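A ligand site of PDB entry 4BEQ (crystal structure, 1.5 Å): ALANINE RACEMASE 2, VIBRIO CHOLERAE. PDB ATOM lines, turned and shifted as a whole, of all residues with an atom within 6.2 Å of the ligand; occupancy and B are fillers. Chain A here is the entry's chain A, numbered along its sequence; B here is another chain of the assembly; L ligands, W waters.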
ATOM      1  N   ILE A  49      -6.349 -25.739  -0.068  1.00  0.00           N
ATOM      2  CA  ILE A  49      -7.477 -25.680   0.864  1.00  0.00           C
ATOM      3  C   ILE A  49      -7.284 -26.688   2.007  1.00  0.00           C
ATOM      4  O   ILE A  49      -7.148 -27.886   1.782  1.00  0.00           O
ATOM      5  CB  ILE A  49      -8.820 -25.893   0.160  1.00  0.00           C
ATOM      6  CG1 ILE A  49      -8.953 -24.888  -1.024  1.00  0.00           C
ATOM      7  CG2 ILE A  49      -9.967 -25.764   1.150  1.00  0.00           C
ATOM      8  CD1 ILE A  49      -8.712 -23.420  -0.597  1.00  0.00           C
ATOM      9  N   LYS A  51      -9.133 -26.693   5.147  1.00  0.00           N
ATOM     10  CA  LYS A  51     -10.241 -26.693   6.085  1.00  0.00           C
ATOM     11  C   LYS A  51     -10.421 -28.065   6.727  1.00  0.00           C
ATOM     12  O   LYS A  51      -9.928 -29.076   6.251  1.00  0.00           O
ATOM     13  CB  LYS A  51     -11.533 -26.269   5.386  1.00  0.00           C
ATOM     14  CG  LYS A  51     -12.040 -27.266   4.359  1.00  0.00           C
ATOM     15  CD  LYS A  51     -12.953 -26.581   3.371  1.00  0.00           C
ATOM     16  CE  LYS A  51     -13.726 -27.569   2.504  1.00  0.00           C
ATOM     17  NZ  LYS A  51     -14.311 -26.793   1.373  1.00  0.00           N
ATOM     18  N   TYR A  55      -8.446 -31.537   6.076  1.00  0.00           N
ATOM     19  CA  TYR A  55      -9.254 -32.691   5.634  1.00  0.00           C
ATOM     20  C   TYR A  55      -8.978 -33.912   6.535  1.00  0.00           C
ATOM     21  O   TYR A  55      -8.922 -35.055   6.081  1.00  0.00           O
ATOM     22  CB  TYR A  55      -9.034 -32.996   4.148  1.00  0.00           C
ATOM     23  CG  TYR A  55      -9.680 -32.029   3.175  1.00  0.00           C
ATOM     24  CD1 TYR A  55      -9.441 -30.677   3.252  1.00  0.00           C
ATOM     25  CD2 TYR A  55     -10.499 -32.492   2.143  1.00  0.00           C
ATOM     26  CE1 TYR A  55     -10.028 -29.790   2.367  1.00  0.00           C
ATOM     27  CE2 TYR A  55     -11.084 -31.619   1.248  1.00  0.00           C
ATOM     28  CZ  TYR A  55     -10.846 -30.271   1.350  1.00  0.00           C
ATOM     29  OH  TYR A  55     -11.393 -29.371   0.457  1.00  0.00           O
ATOM     30  N   VAL A  97     -12.707 -19.900   3.375  1.00  0.00           N
ATOM     31  CA  VAL A  97     -13.425 -20.511   2.265  1.00  0.00           C
ATOM     32  C   VAL A  97     -14.944 -20.529   2.478  1.00  0.00           C
ATOM     33  O   VAL A  97     -15.688 -21.044   1.660  1.00  0.00           O
ATOM     34  CB  VAL A  97     -12.964 -21.950   1.990  1.00  0.00           C
ATOM     35  CG1 VAL A  97     -11.466 -21.976   1.711  1.00  0.00           C
ATOM     36  CG2 VAL A  97     -13.313 -22.839   3.147  1.00  0.00           C
ATOM     37  N   ARG A  98     -15.403 -19.956   3.588  1.00  0.00           N
ATOM     38  CA  ARG A  98     -16.818 -19.951   3.906  1.00  0.00           C
ATOM     39  C   ARG A  98     -17.235 -18.637   4.540  1.00  0.00           C
ATOM     40  O   ARG A  98     -16.399 -17.866   5.023  1.00  0.00           O
ATOM     41  CB  ARG A  98     -17.198 -21.121   4.826  1.00  0.00           C
ATOM     42  CG  ARG A  98     -16.513 -21.110   6.197  1.00  0.00           C
ATOM     43  CD  ARG A  98     -17.338 -21.824   7.266  1.00  0.00           C
ATOM     44  NE  ARG A  98     -16.673 -22.010   8.555  1.00  0.00           N
ATOM     45  CZ  ARG A  98     -16.540 -21.079   9.498  1.00  0.00           C
ATOM     46  NH1 ARG A  98     -16.981 -19.848   9.305  1.00  0.00           N
ATOM     47  NH2 ARG A  98     -15.962 -21.389  10.636  1.00  0.00           N
ATOM     48  N   LEU A 116     -14.501 -13.855   2.966  1.00  0.00           N
ATOM     49  CA  LEU A 116     -15.263 -14.214   1.783  1.00  0.00           C
ATOM     50  C   LEU A 116     -16.667 -13.713   1.983  1.00  0.00           C
ATOM     51  O   LEU A 116     -17.415 -14.239   2.798  1.00  0.00           O
ATOM     52  CB  LEU A 116     -15.305 -15.731   1.627  1.00  0.00           C
ATOM     53  CG  LEU A 116     -16.044 -16.259   0.395  1.00  0.00           C
ATOM     54  CD1 LEU A 116     -15.318 -15.856  -0.888  1.00  0.00           C
ATOM     55  CD2 LEU A 116     -16.207 -17.773   0.474  1.00  0.00           C
ATOM     56  N   MET A 179     -14.938 -14.656  -6.972  1.00  0.00           N
ATOM     57  CA  MET A 179     -14.946 -16.108  -7.080  1.00  0.00           C
ATOM     58  C   MET A 179     -16.350 -16.675  -7.192  1.00  0.00           C
ATOM     59  O   MET A 179     -17.350 -16.019  -6.914  1.00  0.00           O
ATOM     60  CB  MET A 179     -14.246 -16.708  -5.844  1.00  0.00           C
ATOM     61  CG  MET A 179     -14.941 -16.472  -4.494  1.00  0.00           C
ATOM     62  SD  MET A 179     -16.304 -17.583  -4.114  1.00  0.00           S
ATOM     63  CE  MET A 179     -15.473 -19.072  -3.528  1.00  0.00           C
ATOM     64  N   THR A 180     -16.401 -17.945  -7.596  1.00  0.00           N
ATOM     65  CA  THR A 180     -17.590 -18.745  -7.427  1.00  0.00           C
ATOM     66  C   THR A 180     -17.138 -20.174  -7.165  1.00  0.00           C
ATOM     67  O   THR A 180     -15.953 -20.449  -7.065  1.00  0.00           O
ATOM     68  CB  THR A 180     -18.604 -18.621  -8.629  1.00  0.00           C
ATOM     69  OG1 THR A 180     -19.878 -19.131  -8.225  1.00  0.00           O
ATOM     70  CG2 THR A 180     -18.121 -19.344  -9.864  1.00  0.00           C
ATOM     71  N   HIS A 181     -18.110 -21.060  -7.000  1.00  0.00           N
ATOM     72  CA  HIS A 181     -17.860 -22.442  -6.605  1.00  0.00           C
ATOM     73  C   HIS A 181     -18.919 -23.311  -7.270  1.00  0.00           C
ATOM     74  O   HIS A 181     -20.095 -22.955  -7.342  1.00  0.00           O
ATOM     75  CB  HIS A 181     -17.939 -22.520  -5.077  1.00  0.00           C
ATOM     76  CG  HIS A 181     -17.433 -23.793  -4.477  1.00  0.00           C
ATOM     77  ND1 HIS A 181     -16.209 -24.353  -4.800  1.00  0.00           N
ATOM     78  CD2 HIS A 181     -17.954 -24.560  -3.484  1.00  0.00           C
ATOM     79  CE1 HIS A 181     -16.034 -25.440  -4.074  1.00  0.00           C
ATOM     80  NE2 HIS A 181     -17.070 -25.585  -3.274  1.00  0.00           N
ATOM     81  N   TYR A 185     -19.546 -32.358 -10.453  1.00  0.00           N
ATOM     82  CA  TYR A 185     -18.385 -32.730 -11.280  1.00  0.00           C
ATOM     83  C   TYR A 185     -18.800 -32.969 -12.732  1.00  0.00           C
ATOM     84  O   TYR A 185     -18.341 -33.925 -13.364  1.00  0.00           O
ATOM     85  CB  TYR A 185     -17.753 -34.006 -10.733  1.00  0.00           C
ATOM     86  CG  TYR A 185     -17.122 -33.909  -9.347  1.00  0.00           C
ATOM     87  CD1 TYR A 185     -16.790 -32.685  -8.784  1.00  0.00           C
ATOM     88  CD2 TYR A 185     -16.832 -35.054  -8.629  1.00  0.00           C
ATOM     89  CE1 TYR A 185     -16.209 -32.607  -7.524  1.00  0.00           C
ATOM     90  CE2 TYR A 185     -16.254 -34.991  -7.370  1.00  0.00           C
ATOM     91  CZ  TYR A 185     -15.923 -33.755  -6.835  1.00  0.00           C
ATOM     92  OH  TYR A 185     -15.359 -33.673  -5.575  1.00  0.00           O
ATOM     93  N   ALA A 220     -12.105 -22.605  -9.346  1.00  0.00           N
ATOM     94  CA  ALA A 220     -11.870 -24.045  -9.468  1.00  0.00           C
ATOM     95  C   ALA A 220     -11.510 -24.722  -8.162  1.00  0.00           C
ATOM     96  O   ALA A 220     -10.492 -24.415  -7.563  1.00  0.00           O
ATOM     97  CB  ALA A 220     -10.769 -24.305 -10.486  1.00  0.00           C
ATOM     98  N   ASN A 221     -12.334 -25.673  -7.777  1.00  0.00           N
ATOM     99  CA  ASN A 221     -11.960 -26.721  -6.821  1.00  0.00           C
ATOM    100  C   ASN A 221     -11.083 -27.779  -7.504  1.00  0.00           C
ATOM    101  O   ASN A 221     -10.667 -27.602  -8.661  1.00  0.00           O
ATOM    102  CB  ASN A 221     -13.221 -27.333  -6.211  1.00  0.00           C
ATOM    103  CG  ASN A 221     -14.188 -27.954  -7.261  1.00  0.00           C
ATOM    104  OD1 ASN A 221     -13.914 -28.043  -8.464  1.00  0.00           O
ATOM    105  ND2 ASN A 221     -15.351 -28.393  -6.786  1.00  0.00           N
ATOM    106  N   SER A 222     -10.784 -28.872  -6.807  1.00  0.00           N
ATOM    107  CA  SER A 222      -9.909 -29.917  -7.327  1.00  0.00           C
ATOM    108  C   SER A 222     -10.382 -30.424  -8.670  1.00  0.00           C
ATOM    109  O   SER A 222      -9.607 -30.443  -9.638  1.00  0.00           O
ATOM    110  CB  SER A 222      -9.827 -31.117  -6.375  1.00  0.00           C
ATOM    111  OG  SER A 222      -9.284 -30.758  -5.108  1.00  0.00           O
ATOM    112  N   TYR A 223     -11.647 -30.823  -8.721  1.00  0.00           N
ATOM    113  CA  TYR A 223     -12.212 -31.391  -9.943  1.00  0.00           C
ATOM    114  C   TYR A 223     -12.076 -30.430 -11.106  1.00  0.00           C
ATOM    115  O   TYR A 223     -11.595 -30.804 -12.195  1.00  0.00           O
ATOM    116  CB  TYR A 223     -13.702 -31.728  -9.766  1.00  0.00           C
ATOM    117  CG  TYR A 223     -14.267 -32.070 -11.114  1.00  0.00           C
ATOM    118  CD1 TYR A 223     -14.080 -33.316 -11.652  1.00  0.00           C
ATOM    119  CD2 TYR A 223     -14.935 -31.108 -11.863  1.00  0.00           C
ATOM    120  CE1 TYR A 223     -14.529 -33.612 -12.912  1.00  0.00           C
ATOM    121  CE2 TYR A 223     -15.397 -31.410 -13.120  1.00  0.00           C
ATOM    122  CZ  TYR A 223     -15.188 -32.658 -13.627  1.00  0.00           C
ATOM    123  OH  TYR A 223     -15.622 -32.948 -14.914  1.00  0.00           O
ATOM    124  N   ARG A 237      -8.256 -23.582  -6.259  1.00  0.00           N
ATOM    125  CA  ARG A 237      -8.514 -23.871  -4.833  1.00  0.00           C
ATOM    126  C   ARG A 237      -8.631 -25.378  -4.630  1.00  0.00           C
ATOM    127  O   ARG A 237      -9.716 -25.878  -4.281  1.00  0.00           O
ATOM    128  CB  ARG A 237      -9.793 -23.181  -4.344  1.00  0.00           C
ATOM    129  CG  ARG A 237      -9.835 -21.654  -4.444  1.00  0.00           C
ATOM    130  CD  ARG A 237     -11.036 -21.065  -3.723  1.00  0.00           C
ATOM    131  NE  ARG A 237     -12.281 -21.707  -4.152  1.00  0.00           N
ATOM    132  CZ  ARG A 237     -13.038 -21.338  -5.179  1.00  0.00           C
ATOM    133  NH1 ARG A 237     -12.745 -20.269  -5.908  1.00  0.00           N
ATOM    134  NH2 ARG A 237     -14.124 -22.036  -5.468  1.00  0.00           N
ATOM    135  N   PRO A 238      -7.543 -26.098  -4.836  1.00  0.00           N
ATOM    136  CA  PRO A 238      -7.569 -27.551  -4.614  1.00  0.00           C
ATOM    137  C   PRO A 238      -7.532 -27.891  -3.121  1.00  0.00           C
ATOM    138  O   PRO A 238      -6.654 -27.403  -2.400  1.00  0.00           O
ATOM    139  CB  PRO A 238      -6.264 -28.013  -5.286  1.00  0.00           C
ATOM    140  CG  PRO A 238      -5.333 -26.861  -5.142  1.00  0.00           C
ATOM    141  CD  PRO A 238      -6.230 -25.662  -5.358  1.00  0.00           C
ATOM    142  N   GLY A 239      -8.495 -28.687  -2.688  1.00  0.00           N
ATOM    143  CA  GLY A 239      -8.456 -29.331  -1.380  1.00  0.00           C
ATOM    144  C   GLY A 239      -8.284 -30.836  -1.548  1.00  0.00           C
ATOM    145  O   GLY A 239      -7.160 -31.341  -1.483  1.00  0.00           O
ATOM    146  N   GLY A 240      -9.402 -31.553  -1.759  1.00  0.00           N
ATOM    147  CA  GLY A 240      -9.394 -33.000  -1.778  1.00  0.00           C
ATOM    148  C   GLY A 240      -8.288 -33.662  -2.594  1.00  0.00           C
ATOM    149  O   GLY A 240      -7.701 -34.652  -2.148  1.00  0.00           O
ATOM    150  N   VAL A 241      -8.003 -33.177  -3.793  1.00  0.00           N
ATOM    151  CA  VAL A 241      -7.030 -33.870  -4.610  1.00  0.00           C
ATOM    152  C   VAL A 241      -5.639 -33.906  -3.956  1.00  0.00           C
ATOM    153  O   VAL A 241      -4.888 -34.875  -4.132  1.00  0.00           O
ATOM    154  CB  VAL A 241      -6.980 -33.309  -6.059  1.00  0.00           C
ATOM    155  CG1 VAL A 241      -6.407 -31.910  -6.093  1.00  0.00           C
ATOM    156  CG2 VAL A 241      -6.205 -34.239  -6.967  1.00  0.00           C
ATOM    157  N   ASP A 245      -8.222 -37.428  -2.332  1.00  0.00           N
ATOM    158  CA  ASP A 245      -9.660 -37.665  -2.373  1.00  0.00           C
ATOM    159  C   ASP A 245     -10.305 -36.820  -3.466  1.00  0.00           C
ATOM    160  O   ASP A 245     -11.014 -35.860  -3.206  1.00  0.00           O
ATOM    161  CB  ASP A 245     -10.329 -37.313  -1.048  1.00  0.00           C
ATOM    162  CG  ASP A 245     -11.833 -37.555  -1.090  1.00  0.00           C
ATOM    163  OD1 ASP A 245     -12.247 -38.419  -1.887  1.00  0.00           O
ATOM    164  OD2 ASP A 245     -12.589 -36.890  -0.369  1.00  0.00           O
ATOM    165  N   LEU A 246     -10.049 -37.185  -4.718  1.00  0.00           N
ATOM    166  CA  LEU A 246     -10.799 -36.646  -5.851  1.00  0.00           C
ATOM    167  C   LEU A 246     -11.266 -37.862  -6.620  1.00  0.00           C
ATOM    168  O   LEU A 246     -10.471 -38.468  -7.314  1.00  0.00           O
ATOM    169  CB  LEU A 246      -9.916 -35.761  -6.732  1.00  0.00           C
ATOM    170  CG  LEU A 246     -10.593 -35.262  -8.022  1.00  0.00           C
ATOM    171  CD1 LEU A 246     -11.935 -34.626  -7.705  1.00  0.00           C
ATOM    172  CD2 LEU A 246      -9.686 -34.282  -8.699  1.00  0.00           C
ATOM    173  N   TYR B 276     -24.225 -28.832  -2.903  1.00  0.00           N
ATOM    174  CA  TYR B 276     -23.585 -29.797  -3.788  1.00  0.00           C
ATOM    175  C   TYR B 276     -24.628 -30.746  -4.347  1.00  0.00           C
ATOM    176  O   TYR B 276     -25.572 -31.126  -3.667  1.00  0.00           O
ATOM    177  CB  TYR B 276     -22.541 -30.601  -3.022  1.00  0.00           C
ATOM    178  CG  TYR B 276     -21.247 -29.887  -2.761  1.00  0.00           C
ATOM    179  CD1 TYR B 276     -20.432 -29.481  -3.823  1.00  0.00           C
ATOM    180  CD2 TYR B 276     -20.803 -29.651  -1.477  1.00  0.00           C
ATOM    181  CE1 TYR B 276     -19.237 -28.854  -3.598  1.00  0.00           C
ATOM    182  CE2 TYR B 276     -19.598 -29.006  -1.245  1.00  0.00           C
ATOM    183  CZ  TYR B 276     -18.820 -28.605  -2.309  1.00  0.00           C
ATOM    184  OH  TYR B 276     -17.601 -27.999  -2.077  1.00  0.00           O
ATOM    185  N   MET B 324     -18.987 -29.883   3.920  1.00  0.00           N
ATOM    186  CA  MET B 324     -18.002 -30.159   4.956  1.00  0.00           C
ATOM    187  C   MET B 324     -18.102 -29.137   6.092  1.00  0.00           C
ATOM    188  O   MET B 324     -17.938 -29.488   7.291  1.00  0.00           O
ATOM    189  CB  MET B 324     -16.586 -30.129   4.357  1.00  0.00           C
ATOM    190  CG  MET B 324     -15.506 -30.665   5.290  1.00  0.00           C
ATOM    191  SD  MET B 324     -13.878 -30.783   4.521  1.00  0.00           S
ATOM    192  CE  MET B 324     -14.070 -32.173   3.443  1.00  0.00           C
ATOM    193  N   ASN B 325     -18.363 -27.878   5.746  1.00  0.00           N
ATOM    194  CA  ASN B 325     -18.334 -26.794   6.727  1.00  0.00           C
ATOM    195  C   ASN B 325     -19.561 -25.890   6.840  1.00  0.00           C
ATOM    196  O   ASN B 325     -19.586 -25.043   7.728  1.00  0.00           O
ATOM    197  CB  ASN B 325     -17.106 -25.904   6.482  1.00  0.00           C
ATOM    198  CG  ASN B 325     -15.808 -26.633   6.706  1.00  0.00           C
ATOM    199  OD1 ASN B 325     -15.397 -26.893   7.852  1.00  0.00           O
ATOM    200  ND2 ASN B 325     -15.188 -27.020   5.650  1.00  0.00           N
HETATM  201  N1  LIG L   1     -13.493 -23.809  -2.663  1.00  0.00           N
HETATM  202  C1  LIG L   1     -14.390 -23.718  -1.616  1.00  0.00           C
HETATM  203  C2  LIG L   1     -15.209 -22.474  -1.482  1.00  0.00           C
HETATM  204  C3  LIG L   1     -14.511 -24.769  -0.716  1.00  0.00           C
HETATM  205  O1  LIG L   1     -15.436 -24.612   0.293  1.00  0.00           O
HETATM  206  C4  LIG L   1     -13.716 -25.912  -0.887  1.00  0.00           C
HETATM  207  C5  LIG L   1     -13.584 -26.961   0.147  1.00  0.00           C
HETATM  208  C6  LIG L   1     -12.825 -25.982  -1.965  1.00  0.00           C
HETATM  209  C7  LIG L   1     -12.716 -24.926  -2.836  1.00  0.00           C
HETATM  210  C8  LIG L   1     -11.982 -27.218  -2.195  1.00  0.00           C
HETATM  211  O2  LIG L   1     -12.873 -28.255  -2.631  1.00  0.00           O
HETATM  212  P1  LIG L   1     -12.321 -29.673  -3.103  1.00  0.00           P
HETATM  213  O3  LIG L   1     -11.947 -30.461  -1.869  1.00  0.00           O
HETATM  214  O4  LIG L   1     -11.124 -29.396  -3.936  1.00  0.00           O
HETATM  215  O5  LIG L   1     -13.484 -30.313  -3.836  1.00  0.00           O
HETATM  216  O   HOH W   1     -13.234 -31.262  -6.344  1.00  0.00           O
HETATM  217  O   HOH W   2     -14.443 -32.683  -3.455  1.00  0.00           O
HETATM  218  O   HOH W   3     -18.051 -26.051  -0.069  1.00  0.00           O
HETATM  219  O   HOH W   4     -17.235 -23.033   1.422  1.00  0.00           O
HETATM  220  O   HOH W   5     -15.825 -29.103  -4.061  1.00  0.00           O
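The side-chain amino group of Lys 51 is bonded to a carbon (C5) of the ligand, at 1.4 Å.
The backbone NH (N) of Ser 222 lies within hydrogen-bond range of an oxygen (O4) of the ligand (2.9 Å).
OG of Ser 222 is in hydrogen-bond range of O4 of the ligand (2.6 Å).
The side-chain hydroxyl (OH) of Tyr 55 lies within hydrogen-bond range of an oxygen (O3) of the ligand (2.6 Å).
The backbone NH (N) of Gly 240 sits at hydrogen-bond distance from an oxygen (O3) of the ligand (2.8 Å).
NE of Arg 237 sits at hydrogen-bond distance from N1 of the ligand (2.8 Å).
The backbone NH of Gly 239 sits at hydrogen-bond distance from an oxygen (O4) of the ligand (3.0 Å).
A ring nitrogen (ND1) of His 181 sits close to a nitrogen (N1) of the ligand (3.5 Å).
The side-chain hydroxyl (OG) of Ser 222 is in hydrogen-bond range of the backbone NH (N) of Gly 240, at 3.4 Å.
The side-chain hydroxyl (OG) of Ser 222 sits at hydrogen-bond distance from the backbone NH (N) of Val 241 (3.0 Å).
The backbone carbonyl oxygen (O) of Gly 240 sits at hydrogen-bond distance from the backbone NH (N) of Asp 245, 2.8 Å away.
A ring nitrogen (ND1) of His 181 lies within hydrogen-bond range of the guanidinium group (NH2) of Arg 237 (3.2 Å).
The backbone NH of Arg 237 sits at hydrogen-bond distance from the backbone carbonyl oxygen of Ala 220.
The guanidinium group (NH2) of Arg 237 sits at hydrogen-bond distance from the backbone carbonyl oxygen (O) of Thr 180.
OH of Tyr 276 of chain B sits at hydrogen-bond distance from NE2 of His 181.
N of Ile 49 sits at hydrogen-bond distance from O of Pro 238, at 2.9 Å.
Merely in contact with the ligand: Ile 49, Val 97, Met 179, Asn 221 and Pro 238.
Hydrophobic or aromatic side chains that line the ligand: Ile 49, Tyr 55, Val 97, Met 179 and His 181.
Within 4 Å of the ligand: Ile 49, Lys 51, Tyr 55, Val 97, Met 179, His 181, Asn 221, Ser 222, Arg 237, Pro 238, Gly 239 and Gly 240.
The nearest printed residue that does not touch the ligand is Tyr 185 (4.2 Å).
Water W2 bridges the side-chain hydroxyl of Tyr 185 (2.5 Å) and an oxygen (O5) of the ligand (2.6 Å).
Water W5 lies within hydrogen-bond range of O5 of the ligand (2.6 Å), ND2 of Asn 221 (2.9 Å) and OH of Tyr 276 of chain B (2.9 Å).
Water W4 lies within hydrogen-bond range of the backbone carbonyl oxygen (O) of Val 97 (2.5 Å) and an oxygen (O1) of the ligand (2.6 Å).
Water W1 lies within hydrogen-bond range of an oxygen (O5) of the ligand (2.7 Å), the backbone NH (N) of Tyr 223 (2.9 Å), the side-chain hydroxyl (OH) of Tyr 185 (3.3 Å) and the backbone NH (N) of Ser 222 (3.5 Å).
Water W3 lies within hydrogen-bond range of OH of Tyr 276 of chain B (2.8 Å), O1 of the ligand (3.0 Å) and NE2 of His 181 (3.4 Å).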
